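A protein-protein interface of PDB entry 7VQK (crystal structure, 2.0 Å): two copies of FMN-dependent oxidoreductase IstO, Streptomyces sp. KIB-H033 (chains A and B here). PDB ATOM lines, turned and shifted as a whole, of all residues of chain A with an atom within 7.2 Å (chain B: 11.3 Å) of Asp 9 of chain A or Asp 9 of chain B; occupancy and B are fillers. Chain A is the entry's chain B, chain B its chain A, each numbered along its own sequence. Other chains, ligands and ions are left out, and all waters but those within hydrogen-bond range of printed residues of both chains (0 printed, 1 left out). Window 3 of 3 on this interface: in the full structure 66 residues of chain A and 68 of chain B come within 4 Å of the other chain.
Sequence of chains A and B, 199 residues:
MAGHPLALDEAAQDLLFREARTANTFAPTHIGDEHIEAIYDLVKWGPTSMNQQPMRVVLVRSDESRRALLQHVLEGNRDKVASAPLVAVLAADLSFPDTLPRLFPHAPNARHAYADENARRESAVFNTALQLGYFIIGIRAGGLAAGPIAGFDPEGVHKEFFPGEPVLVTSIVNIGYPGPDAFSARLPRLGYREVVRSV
The backbone NH (N) of Ala 7 of chain B lies within hydrogen-bond range of the backbone carbonyl oxygen (O) of Ala 141 of chain A (2.8 Å). The backbone carbonyl oxygen (O) of Ala 141 of chain B lies within hydrogen-bond range of the backbone NH (N) of Ala 7 of chain A, 2.8 Å away. The side-chain carboxylate (OD2) of Asp 9 of chain A sits close to the side-chain carboxylate (OD2) of Asp 9 of chain B, 3.3 Å away. O of Ala 141 of chain B is in hydrogen-bond range of N of Leu 8 of chain A (3.0 Å). N of Leu 8 of chain B lies within hydrogen-bond range of O of Ala 141 of chain A (3.1 Å).
OD1 of Asp 9 of chain A lies within hydrogen-bond range of N of Ala 11 of chain A (3.0 Å). O of Leu 8 of chain A lies within hydrogen-bond range of NE2 of Gln 13 of chain A, at 2.6 Å. The side-chain carboxylate (OD1) of Asp 9 of chain B is in hydrogen-bond range of the backbone NH (N) of Ala 12 of chain B, at 2.7 Å. O of Leu 8 of chain B sits at hydrogen-bond distance from NE2 of Gln 13 of chain B, at 2.6 Å. The backbone carbonyl oxygen (O) of Gln 13 of chain B is in hydrogen-bond range of the backbone NH (N) of Arg 18 of chain B, 3.0 Å away. The backbone carbonyl oxygen (O) of Leu 16 of chain B sits at hydrogen-bond distance from the guanidinium group (NH1) of Arg 140 of chain B (2.8 Å).
Among the printed residues, merely in contact across the chains: Leu 6 of chain A with Ala 38 of chain B (3.98 Å), Leu 6 of chain A with Ala 141 of chain B (3.7 Å), Leu 6 of chain A with Gly 142 of chain B (3.8 Å), Ala 7 of chain A with Gly 143 of chain B (3.8 Å), Leu 8 of chain A with Ala 12 of chain B (3.7 Å), Leu 8 of chain A with Leu 15 of chain B (3.7 Å), Leu 8 of chain A with Leu 16 of chain B (3.995 Å), Ala 12 of chain A with Leu 8 of chain B (3.7 Å), Ala 12 of chain A with Ala 12 of chain B (3.8 Å), Gln 13 of chain A with Leu 42 of chain B (3.8 Å), Leu 15 of chain A with Ala 7 of chain B (3.99 Å), Leu 15 of chain A with Leu 8 of chain B (3.7 Å), Leu 42 of chain A with Leu 6 of chain B (3.9 Å), Leu 42 of chain A with Gln 13 of chain B (3.7 Å), Leu 42 of chain A with Phe 17 of chain B (3.4 Å), Leu 42 of chain A with Arg 18 of chain B (3.8 Å) and Ala 141 of chain A with Leu 6 of chain B (3.6 Å).
Printed residues of chain B within 4 Å of Leu 6 of chain A: Ala 38, Ala 141 and Gly 142. Of chain B, only Asp 9 comes within 4 Å of Asp 9 of chain A. No residue of chain B comes within 4 Å of Glu 10 of chain A. No residue of chain B comes within 4 Å of Ala 11 of chain A. Of chain B, only Leu 8 (3.7 Å) and Ala 12 (3.8 Å) come within 4 Å of Ala 12 of chain A. Of the printed residues of chain A, Leu 6 of chain B touches Leu 42 and Ala 141. Of the printed residues of chain A, Asp 9 of chain B touches Asp 9 (3.3 Å). Printed residues of chain A within 4 Å of Leu 15 of chain B: Leu 8 (3.7 Å). Of the printed residues of chain A, Leu 16 of chain B touches Leu 8. Glu 19 of chain B touches none of the printed residues of chain A. Arg 140 of chain B touches none of the printed residues of chain A.
Printed residues of chain A that touch a printed residue of chain B: Leu 6, Ala 7, Leu 8, Asp 9, Ala 12, Gln 13, Leu 15, Leu 42 and Ala 141. Hydrophobic or aromatic side chains of chain A that line the printed part of chain B: Leu 6, Ala 7, Leu 8, Ala 12, Leu 15, Leu 42 and Ala 141. Of the 23 printed residues of chain B, 15 touch a printed residue of chain A. Printed residues of chain B that touch a printed residue of chain A: Leu 6, Ala 7, Leu 8, Asp 9, Ala 12, Gln 13, Leu 15, Leu 16, Phe 17, Arg 18, Ala 38, Leu 42, Ala 141, Gly 142 and Gly 143. Hydrophobic or aromatic side chains of chain B within 4 Å of the printed part of chain A: Leu 6, Ala 7, Leu 8, Ala 12, Leu 15, Leu 16, Phe 17, Ala 38, Leu 42 and Ala 141. Among the printed residues, 22 pairs touch across the chains.
Leu 8 of chain A touches Leu 15 of chain B, and with the chains exchanged Leu 15 of chain A touches Leu 8 of chain B. Leu 8 of chain A touches Ala 141 of chain B, and with the chains exchanged Ala 141 of chain A touches Leu 8 of chain B. Asp 9 of chain A touches its own counterpart, Asp 9 of chain B. Gln 13 of chain A touches Leu 42 of chain B, and with the chains exchanged Leu 42 of chain A touches Gln 13 of chain B. Of the 22 pairs that touch across the chains among the printed residues, 14 have their exchanged pair printed and touching as well.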
ATOM      1  N   LEU A   6       9.953 -35.451 -31.568  1.00  0.00           N
ATOM      2  CA  LEU A   6      10.092 -34.004 -31.420  1.00  0.00           C
ATOM      3  C   LEU A   6      10.978 -33.686 -30.224  1.00  0.00           C
ATOM      4  O   LEU A   6      10.809 -34.270 -29.151  1.00  0.00           O
ATOM      5  CB  LEU A   6       8.730 -33.334 -31.261  1.00  0.00           C
ATOM      6  CG  LEU A   6       7.806 -33.412 -32.473  1.00  0.00           C
ATOM      7  CD1 LEU A   6       6.561 -32.576 -32.233  1.00  0.00           C
ATOM      8  CD2 LEU A   6       8.538 -32.949 -33.719  1.00  0.00           C
ATOM      9  N   ALA A   7      11.943 -32.777 -30.420  1.00  0.00           N
ATOM     10  CA  ALA A   7      12.776 -32.324 -29.309  1.00  0.00           C
ATOM     11  C   ALA A   7      12.047 -31.312 -28.425  1.00  0.00           C
ATOM     12  O   ALA A   7      12.267 -31.272 -27.211  1.00  0.00           O
ATOM     13  CB  ALA A   7      14.077 -31.711 -29.840  1.00  0.00           C
ATOM     14  N   LEU A   8      11.188 -30.488 -29.009  1.00  0.00           N
ATOM     15  CA  LEU A   8      10.441 -29.511 -28.230  1.00  0.00           C
ATOM     16  C   LEU A   8       9.498 -30.225 -27.265  1.00  0.00           C
ATOM     17  O   LEU A   8       8.730 -31.100 -27.670  1.00  0.00           O
ATOM     18  CB  LEU A   8       9.662 -28.602 -29.179  1.00  0.00           C
ATOM     19  CG  LEU A   8       8.895 -27.431 -28.574  1.00  0.00           C
ATOM     20  CD1 LEU A   8       9.875 -26.380 -28.067  1.00  0.00           C
ATOM     21  CD2 LEU A   8       7.961 -26.855 -29.629  1.00  0.00           C
ATOM     22  N   ASP A   9       9.539 -29.852 -25.987  1.00  0.00           N
ATOM     23  CA  ASP A   9       8.722 -30.585 -25.024  1.00  0.00           C
ATOM     24  C   ASP A   9       7.231 -30.292 -25.213  1.00  0.00           C
ATOM     25  O   ASP A   9       6.830 -29.310 -25.847  1.00  0.00           O
ATOM     26  CB  ASP A   9       9.167 -30.292 -23.586  1.00  0.00           C
ATOM     27  CG  ASP A   9       8.775 -28.902 -23.094  1.00  0.00           C
ATOM     28  OD1 ASP A   9       7.604 -28.497 -23.225  1.00  0.00           O
ATOM     29  OD2 ASP A   9       9.646 -28.223 -22.526  1.00  0.00           O
ATOM     30  N   GLU A  10       6.398 -31.176 -24.644  1.00  0.00           N
ATOM     31  CA  GLU A  10       4.965 -31.135 -24.919  1.00  0.00           C
ATOM     32  C   GLU A  10       4.329 -29.825 -24.459  1.00  0.00           C
ATOM     33  O   GLU A  10       3.438 -29.294 -25.133  1.00  0.00           O
ATOM     34  CB  GLU A  10       4.259 -32.325 -24.260  1.00  0.00           C
ATOM     35  CG  GLU A  10       2.830 -32.542 -24.774  1.00  0.00           C
ATOM     36  CD  GLU A  10       1.845 -32.993 -23.700  1.00  0.00           C
ATOM     37  OE1 GLU A  10       2.084 -34.058 -23.094  1.00  0.00           O
ATOM     38  OE2 GLU A  10       0.818 -32.305 -23.484  1.00  0.00           O
ATOM     39  N   ALA A  11       4.737 -29.301 -23.303  1.00  0.00           N
ATOM     40  CA  ALA A  11       4.106 -28.067 -22.835  1.00  0.00           C
ATOM     41  C   ALA A  11       4.400 -26.912 -23.786  1.00  0.00           C
ATOM     42  O   ALA A  11       3.527 -26.063 -24.036  1.00  0.00           O
ATOM     43  CB  ALA A  11       4.559 -27.728 -21.415  1.00  0.00           C
ATOM     44  N   ALA A  12       5.626 -26.851 -24.322  1.00  0.00           N
ATOM     45  CA  ALA A  12       5.930 -25.825 -25.316  1.00  0.00           C
ATOM     46  C   ALA A  12       5.156 -26.070 -26.607  1.00  0.00           C
ATOM     47  O   ALA A  12       4.696 -25.119 -27.251  1.00  0.00           O
ATOM     48  CB  ALA A  12       7.435 -25.775 -25.598  1.00  0.00           C
ATOM     49  N   GLN A  13       5.014 -27.341 -27.001  1.00  0.00           N
ATOM     50  CA  GLN A  13       4.229 -27.673 -28.184  1.00  0.00           C
ATOM     51  C   GLN A  13       2.803 -27.166 -28.044  1.00  0.00           C
ATOM     52  O   GLN A  13       2.226 -26.641 -29.003  1.00  0.00           O
ATOM     53  CB  GLN A  13       4.219 -29.190 -28.414  1.00  0.00           C
ATOM     54  CG  GLN A  13       5.532 -29.809 -28.884  1.00  0.00           C
ATOM     55  CD  GLN A  13       5.416 -31.327 -29.027  1.00  0.00           C
ATOM     56  OE1 GLN A  13       4.393 -31.844 -29.489  1.00  0.00           O
ATOM     57  NE2 GLN A  13       6.453 -32.045 -28.613  1.00  0.00           N
ATOM     58  N   ASP A  14       2.215 -27.335 -26.855  1.00  0.00           N
ATOM     59  CA  ASP A  14       0.836 -26.913 -26.619  1.00  0.00           C
ATOM     60  C   ASP A  14       0.715 -25.396 -26.639  1.00  0.00           C
ATOM     61  O   ASP A  14      -0.191 -24.842 -27.274  1.00  0.00           O
ATOM     62  CB  ASP A  14       0.332 -27.452 -25.273  1.00  0.00           C
ATOM     63  CG  ASP A  14       0.116 -28.964 -25.278  1.00  0.00           C
ATOM     64  OD1 ASP A  14       0.008 -29.545 -26.371  1.00  0.00           O
ATOM     65  OD2 ASP A  14       0.050 -29.566 -24.180  1.00  0.00           O
ATOM     66  N   LEU A  15       1.602 -24.709 -25.916  1.00  0.00           N
ATOM     67  CA  LEU A  15       1.546 -23.249 -25.844  1.00  0.00           C
ATOM     68  C   LEU A  15       1.618 -22.611 -27.228  1.00  0.00           C
ATOM     69  O   LEU A  15       0.883 -21.658 -27.524  1.00  0.00           O
ATOM     70  CB  LEU A  15       2.690 -22.732 -24.972  1.00  0.00           C
ATOM     71  CG  LEU A  15       2.768 -21.216 -24.747  1.00  0.00           C
ATOM     72  CD1 LEU A  15       1.640 -20.734 -23.817  1.00  0.00           C
ATOM     73  CD2 LEU A  15       4.145 -20.835 -24.188  1.00  0.00           C
ATOM     74  N   LEU A  42      12.699 -12.157 -28.812  1.00  0.00           N
ATOM     75  CA  LEU A  42      12.749 -13.596 -29.059  1.00  0.00           C
ATOM     76  C   LEU A  42      12.671 -13.918 -30.544  1.00  0.00           C
ATOM     77  O   LEU A  42      13.506 -14.668 -31.069  1.00  0.00           O
ATOM     78  CB  LEU A  42      11.605 -14.302 -28.318  1.00  0.00           C
ATOM     79  CG  LEU A  42      11.395 -15.783 -28.644  1.00  0.00           C
ATOM     80  CD1 LEU A  42      12.571 -16.614 -28.129  1.00  0.00           C
ATOM     81  CD2 LEU A  42      10.085 -16.292 -28.037  1.00  0.00           C
ATOM     82  N   ALA A 141       4.147 -17.248 -27.366  1.00  0.00           N
ATOM     83  CA  ALA A 141       5.238 -17.461 -26.415  1.00  0.00           C
ATOM     84  C   ALA A 141       5.164 -16.487 -25.250  1.00  0.00           C
ATOM     85  O   ALA A 141       5.612 -16.810 -24.144  1.00  0.00           O
ATOM     86  CB  ALA A 141       6.598 -17.319 -27.108  1.00  0.00           C
ATOM     87  N   PRO B   5       8.782 -11.641 -19.229  1.00  0.00           N
ATOM     88  CA  PRO B   5       7.341 -11.845 -19.441  1.00  0.00           C
ATOM     89  C   PRO B   5       7.017 -12.896 -20.499  1.00  0.00           C
ATOM     90  O   PRO B   5       5.970 -12.801 -21.147  1.00  0.00           O
ATOM     91  CB  PRO B   5       6.847 -10.460 -19.904  1.00  0.00           C
ATOM     92  CG  PRO B   5       8.069  -9.539 -19.864  1.00  0.00           C
ATOM     93  CD  PRO B   5       9.265 -10.439 -19.920  1.00  0.00           C
ATOM     94  N   LEU B   6       7.889 -13.880 -20.692  1.00  0.00           N
ATOM     95  CA  LEU B   6       7.629 -14.955 -21.642  1.00  0.00           C
ATOM     96  C   LEU B   6       7.143 -16.189 -20.896  1.00  0.00           C
ATOM     97  O   LEU B   6       7.787 -16.635 -19.943  1.00  0.00           O
ATOM     98  CB  LEU B   6       8.880 -15.286 -22.457  1.00  0.00           C
ATOM     99  CG  LEU B   6       9.347 -14.202 -23.434  1.00  0.00           C
ATOM    100  CD1 LEU B   6      10.347 -14.786 -24.419  1.00  0.00           C
ATOM    101  CD2 LEU B   6       8.184 -13.534 -24.173  1.00  0.00           C
ATOM    102  N   ALA B   7       6.008 -16.736 -21.333  1.00  0.00           N
ATOM    103  CA  ALA B   7       5.546 -18.005 -20.783  1.00  0.00           C
ATOM    104  C   ALA B   7       6.363 -19.189 -21.305  1.00  0.00           C
ATOM    105  O   ALA B   7       6.482 -20.211 -20.618  1.00  0.00           O
ATOM    106  CB  ALA B   7       4.067 -18.191 -21.108  1.00  0.00           C
ATOM    107  N   LEU B   8       6.913 -19.082 -22.514  1.00  0.00           N
ATOM    108  CA  LEU B   8       7.718 -20.154 -23.093  1.00  0.00           C
ATOM    109  C   LEU B   8       9.014 -20.328 -22.311  1.00  0.00           C
ATOM    110  O   LEU B   8       9.745 -19.357 -22.086  1.00  0.00           O
ATOM    111  CB  LEU B   8       8.037 -19.828 -24.548  1.00  0.00           C
ATOM    112  CG  LEU B   8       8.717 -20.927 -25.358  1.00  0.00           C
ATOM    113  CD1 LEU B   8       7.763 -22.129 -25.543  1.00  0.00           C
ATOM    114  CD2 LEU B   8       9.189 -20.376 -26.702  1.00  0.00           C
ATOM    115  N   ASP B   9       9.317 -21.557 -21.904  1.00  0.00           N
ATOM    116  CA  ASP B   9      10.493 -21.709 -21.059  1.00  0.00           C
ATOM    117  C   ASP B   9      11.774 -21.467 -21.860  1.00  0.00           C
ATOM    118  O   ASP B   9      11.778 -21.424 -23.094  1.00  0.00           O
ATOM    119  CB  ASP B   9      10.494 -23.071 -20.352  1.00  0.00           C
ATOM    120  CG  ASP B   9      10.839 -24.238 -21.263  1.00  0.00           C
ATOM    121  OD1 ASP B   9      11.630 -24.104 -22.226  1.00  0.00           O
ATOM    122  OD2 ASP B   9      10.298 -25.328 -20.998  1.00  0.00           O
ATOM    123  N   GLU B  10      12.869 -21.275 -21.127  1.00  0.00           N
ATOM    124  CA  GLU B  10      14.118 -20.838 -21.741  1.00  0.00           C
ATOM    125  C   GLU B  10      14.688 -21.886 -22.693  1.00  0.00           C
ATOM    126  O   GLU B  10      15.208 -21.545 -23.762  1.00  0.00           O
ATOM    127  CB  GLU B  10      15.133 -20.490 -20.651  1.00  0.00           C
ATOM    128  CG  GLU B  10      15.132 -19.012 -20.307  1.00  0.00           C
ATOM    129  CD  GLU B  10      15.672 -18.713 -18.923  1.00  0.00           C
ATOM    130  OE1 GLU B  10      16.507 -19.495 -18.419  1.00  0.00           O
ATOM    131  OE2 GLU B  10      15.259 -17.684 -18.342  1.00  0.00           O
ATOM    132  N   ALA B  11      14.617 -23.167 -22.319  1.00  0.00           N
ATOM    133  CA  ALA B  11      15.123 -24.210 -23.207  1.00  0.00           C
ATOM    134  C   ALA B  11      14.377 -24.200 -24.537  1.00  0.00           C
ATOM    135  O   ALA B  11      14.991 -24.347 -25.602  1.00  0.00           O
ATOM    136  CB  ALA B  11      15.011 -25.580 -22.535  1.00  0.00           C
ATOM    137  N   ALA B  12      13.054 -24.012 -24.499  1.00  0.00           N
ATOM    138  CA  ALA B  12      12.286 -23.929 -25.738  1.00  0.00           C
ATOM    139  C   ALA B  12      12.638 -22.670 -26.526  1.00  0.00           C
ATOM    140  O   ALA B  12      12.775 -22.720 -27.758  1.00  0.00           O
ATOM    141  CB  ALA B  12      10.786 -23.978 -25.434  1.00  0.00           C
ATOM    142  N   GLN B  13      12.789 -21.529 -25.840  1.00  0.00           N
ATOM    143  CA  GLN B  13      13.202 -20.304 -26.527  1.00  0.00           C
ATOM    144  C   GLN B  13      14.497 -20.525 -27.297  1.00  0.00           C
ATOM    145  O   GLN B  13      14.627 -20.087 -28.446  1.00  0.00           O
ATOM    146  CB  GLN B  13      13.373 -19.152 -25.532  1.00  0.00           C
ATOM    147  CG  GLN B  13      12.103 -18.714 -24.803  1.00  0.00           C
ATOM    148  CD  GLN B  13      12.375 -17.639 -23.752  1.00  0.00           C
ATOM    149  OE1 GLN B  13      13.143 -16.710 -23.989  1.00  0.00           O
ATOM    150  NE2 GLN B  13      11.764 -17.780 -22.580  1.00  0.00           N
ATOM    151  N   ASP B  14      15.461 -21.216 -26.682  1.00  0.00           N
ATOM    152  CA  ASP B  14      16.753 -21.441 -27.324  1.00  0.00           C
ATOM    153  C   ASP B  14      16.632 -22.379 -28.516  1.00  0.00           C
ATOM    154  O   ASP B  14      17.232 -22.133 -29.571  1.00  0.00           O
ATOM    155  CB  ASP B  14      17.745 -22.012 -26.314  1.00  0.00           C
ATOM    156  CG  ASP B  14      18.201 -20.983 -25.301  1.00  0.00           C
ATOM    157  OD1 ASP B  14      17.911 -19.782 -25.495  1.00  0.00           O
ATOM    158  OD2 ASP B  14      18.854 -21.384 -24.315  1.00  0.00           O
ATOM    159  N   LEU B  15      15.875 -23.469 -28.361  1.00  0.00           N
ATOM    160  CA  LEU B  15      15.756 -24.448 -29.435  1.00  0.00           C
ATOM    161  C   LEU B  15      15.109 -23.840 -30.670  1.00  0.00           C
ATOM    162  O   LEU B  15      15.540 -24.107 -31.796  1.00  0.00           O
ATOM    163  CB  LEU B  15      14.943 -25.655 -28.960  1.00  0.00           C
ATOM    164  CG  LEU B  15      14.696 -26.774 -29.983  1.00  0.00           C
ATOM    165  CD1 LEU B  15      15.920 -27.650 -30.166  1.00  0.00           C
ATOM    166  CD2 LEU B  15      13.483 -27.628 -29.579  1.00  0.00           C
ATOM    167  N   LEU B  16      14.066 -23.030 -30.485  1.00  0.00           N
ATOM    168  CA  LEU B  16      13.320 -22.534 -31.637  1.00  0.00           C
ATOM    169  C   LEU B  16      13.896 -21.245 -32.219  1.00  0.00           C
ATOM    170  O   LEU B  16      13.716 -20.984 -33.417  1.00  0.00           O
ATOM    171  CB  LEU B  16      11.855 -22.304 -31.257  1.00  0.00           C
ATOM    172  CG  LEU B  16      11.125 -23.524 -30.697  1.00  0.00           C
ATOM    173  CD1 LEU B  16       9.651 -23.190 -30.462  1.00  0.00           C
ATOM    174  CD2 LEU B  16      11.308 -24.742 -31.621  1.00  0.00           C
ATOM    175  N   PHE B  17      14.574 -20.431 -31.413  1.00  0.00           N
ATOM    176  CA  PHE B  17      14.940 -19.088 -31.856  1.00  0.00           C
ATOM    177  C   PHE B  17      16.347 -18.662 -31.442  1.00  0.00           C
ATOM    178  O   PHE B  17      17.177 -18.328 -32.294  1.00  0.00           O
ATOM    179  CB  PHE B  17      13.936 -18.058 -31.308  1.00  0.00           C
ATOM    180  CG  PHE B  17      12.602 -18.059 -32.010  1.00  0.00           C
ATOM    181  CD1 PHE B  17      12.457 -17.479 -33.269  1.00  0.00           C
ATOM    182  CD2 PHE B  17      11.477 -18.605 -31.386  1.00  0.00           C
ATOM    183  CE1 PHE B  17      11.211 -17.467 -33.914  1.00  0.00           C
ATOM    184  CE2 PHE B  17      10.219 -18.597 -32.020  1.00  0.00           C
ATOM    185  CZ  PHE B  17      10.086 -18.035 -33.287  1.00  0.00           C
ATOM    186  N   ARG B  18      16.624 -18.641 -30.135  1.00  0.00           N
ATOM    187  CA  ARG B  18      17.800 -17.919 -29.654  1.00  0.00           C
ATOM    188  C   ARG B  18      19.093 -18.626 -30.037  1.00  0.00           C
ATOM    189  O   ARG B  18      20.087 -17.970 -30.371  1.00  0.00           O
ATOM    190  CB  ARG B  18      17.727 -17.731 -28.141  1.00  0.00           C
ATOM    191  CG  ARG B  18      16.539 -16.908 -27.665  1.00  0.00           C
ATOM    192  CD  ARG B  18      16.719 -16.489 -26.219  1.00  0.00           C
ATOM    193  NE  ARG B  18      15.539 -15.803 -25.711  1.00  0.00           N
ATOM    194  CZ  ARG B  18      15.267 -14.521 -25.918  1.00  0.00           C
ATOM    195  NH1 ARG B  18      16.091 -13.742 -26.595  1.00  0.00           N
ATOM    196  NH2 ARG B  18      14.127 -14.014 -25.442  1.00  0.00           N
ATOM    197  N   GLU B  19      19.113 -19.958 -29.985  1.00  0.00           N
ATOM    198  CA  GLU B  19      20.318 -20.705 -30.341  1.00  0.00           C
ATOM    199  C   GLU B  19      20.154 -21.476 -31.642  1.00  0.00           C
ATOM    200  O   GLU B  19      21.018 -22.283 -31.993  1.00  0.00           O
ATOM    201  CB  GLU B  19      20.719 -21.644 -29.202  1.00  0.00           C
ATOM    202  CG  GLU B  19      21.080 -20.900 -27.904  1.00  0.00           C
ATOM    203  CD  GLU B  19      22.214 -19.905 -28.100  1.00  0.00           C
ATOM    204  OE1 GLU B  19      23.099 -20.180 -28.939  1.00  0.00           O
ATOM    205  OE2 GLU B  19      22.221 -18.848 -27.421  1.00  0.00           O
ATOM    206  N   ALA B  38       5.867 -35.974 -37.969  1.00  0.00           N
ATOM    207  CA  ALA B  38       5.717 -35.380 -36.641  1.00  0.00           C
ATOM    208  C   ALA B  38       5.805 -33.861 -36.702  1.00  0.00           C
ATOM    209  O   ALA B  38       5.137 -33.161 -35.928  1.00  0.00           O
ATOM    210  CB  ALA B  38       6.777 -35.928 -35.681  1.00  0.00           C
ATOM    211  N   LEU B  42       2.635 -31.039 -35.899  1.00  0.00           N
ATOM    212  CA  LEU B  42       2.728 -29.954 -34.930  1.00  0.00           C
ATOM    213  C   LEU B  42       2.334 -28.623 -35.557  1.00  0.00           C
ATOM    214  O   LEU B  42       1.445 -27.931 -35.047  1.00  0.00           O
ATOM    215  CB  LEU B  42       4.147 -29.872 -34.353  1.00  0.00           C
ATOM    216  CG  LEU B  42       4.436 -28.687 -33.421  1.00  0.00           C
ATOM    217  CD1 LEU B  42       3.598 -28.773 -32.119  1.00  0.00           C
ATOM    218  CD2 LEU B  42       5.917 -28.613 -33.096  1.00  0.00           C
ATOM    219  N   ILE B 137      10.134 -23.217 -37.832  1.00  0.00           N
ATOM    220  CA  ILE B 137      10.074 -23.468 -36.393  1.00  0.00           C
ATOM    221  C   ILE B 137       9.836 -24.952 -36.123  1.00  0.00           C
ATOM    222  O   ILE B 137      10.410 -25.534 -35.194  1.00  0.00           O
ATOM    223  CB  ILE B 137       8.983 -22.595 -35.738  1.00  0.00           C
ATOM    224  CG1 ILE B 137       9.227 -21.107 -36.031  1.00  0.00           C
ATOM    225  CG2 ILE B 137       8.909 -22.871 -34.230  1.00  0.00           C
ATOM    226  CD1 ILE B 137      10.689 -20.732 -36.086  1.00  0.00           C
ATOM    227  N   GLY B 138       8.982 -25.585 -36.925  1.00  0.00           N
ATOM    228  CA  GLY B 138       8.720 -27.006 -36.728  1.00  0.00           C
ATOM    229  C   GLY B 138       9.946 -27.874 -36.978  1.00  0.00           C
ATOM    230  O   GLY B 138      10.196 -28.835 -36.245  1.00  0.00           O
ATOM    231  N   ARG B 140      13.034 -27.024 -36.505  1.00  0.00           N
ATOM    232  CA  ARG B 140      13.819 -26.888 -35.284  1.00  0.00           C
ATOM    233  C   ARG B 140      13.164 -27.626 -34.119  1.00  0.00           C
ATOM    234  O   ARG B 140      13.856 -28.225 -33.286  1.00  0.00           O
ATOM    235  CB  ARG B 140      14.013 -25.406 -34.958  1.00  0.00           C
ATOM    236  CG  ARG B 140      14.861 -24.682 -35.994  1.00  0.00           C
ATOM    237  CD  ARG B 140      14.526 -23.192 -36.040  1.00  0.00           C
ATOM    238  NE  ARG B 140      15.456 -22.450 -36.889  1.00  0.00           N
ATOM    239  CZ  ARG B 140      15.665 -21.142 -36.775  1.00  0.00           C
ATOM    240  NH1 ARG B 140      14.994 -20.413 -35.896  1.00  0.00           N
ATOM    241  NH2 ARG B 140      16.600 -20.562 -37.528  1.00  0.00           N
ATOM    242  N   ALA B 141      11.835 -27.590 -34.037  1.00  0.00           N
ATOM    243  CA  ALA B 141      11.153 -28.314 -32.969  1.00  0.00           C
ATOM    244  C   ALA B 141      11.451 -29.807 -33.045  1.00  0.00           C
ATOM    245  O   ALA B 141      11.469 -30.492 -32.017  1.00  0.00           O
ATOM    246  CB  ALA B 141       9.647 -28.077 -33.040  1.00  0.00           C
ATOM    247  N   GLY B 142      11.680 -30.323 -34.246  1.00  0.00           N
ATOM    248  CA  GLY B 142      12.024 -31.713 -34.471  1.00  0.00           C
ATOM    249  C   GLY B 142      13.473 -32.043 -34.218  1.00  0.00           C
ATOM    250  O   GLY B 142      13.930 -33.129 -34.586  1.00  0.00           O
ATOM    251  N   GLY B 143      14.225 -31.120 -33.618  1.00  0.00           N
ATOM    252  CA  GLY B 143      15.644 -31.337 -33.387  1.00  0.00           C
ATOM    253  C   GLY B 143      16.523 -31.239 -34.614  1.00  0.00           C
ATOM    254  O   GLY B 143      17.692 -31.641 -34.557  1.00  0.00           O
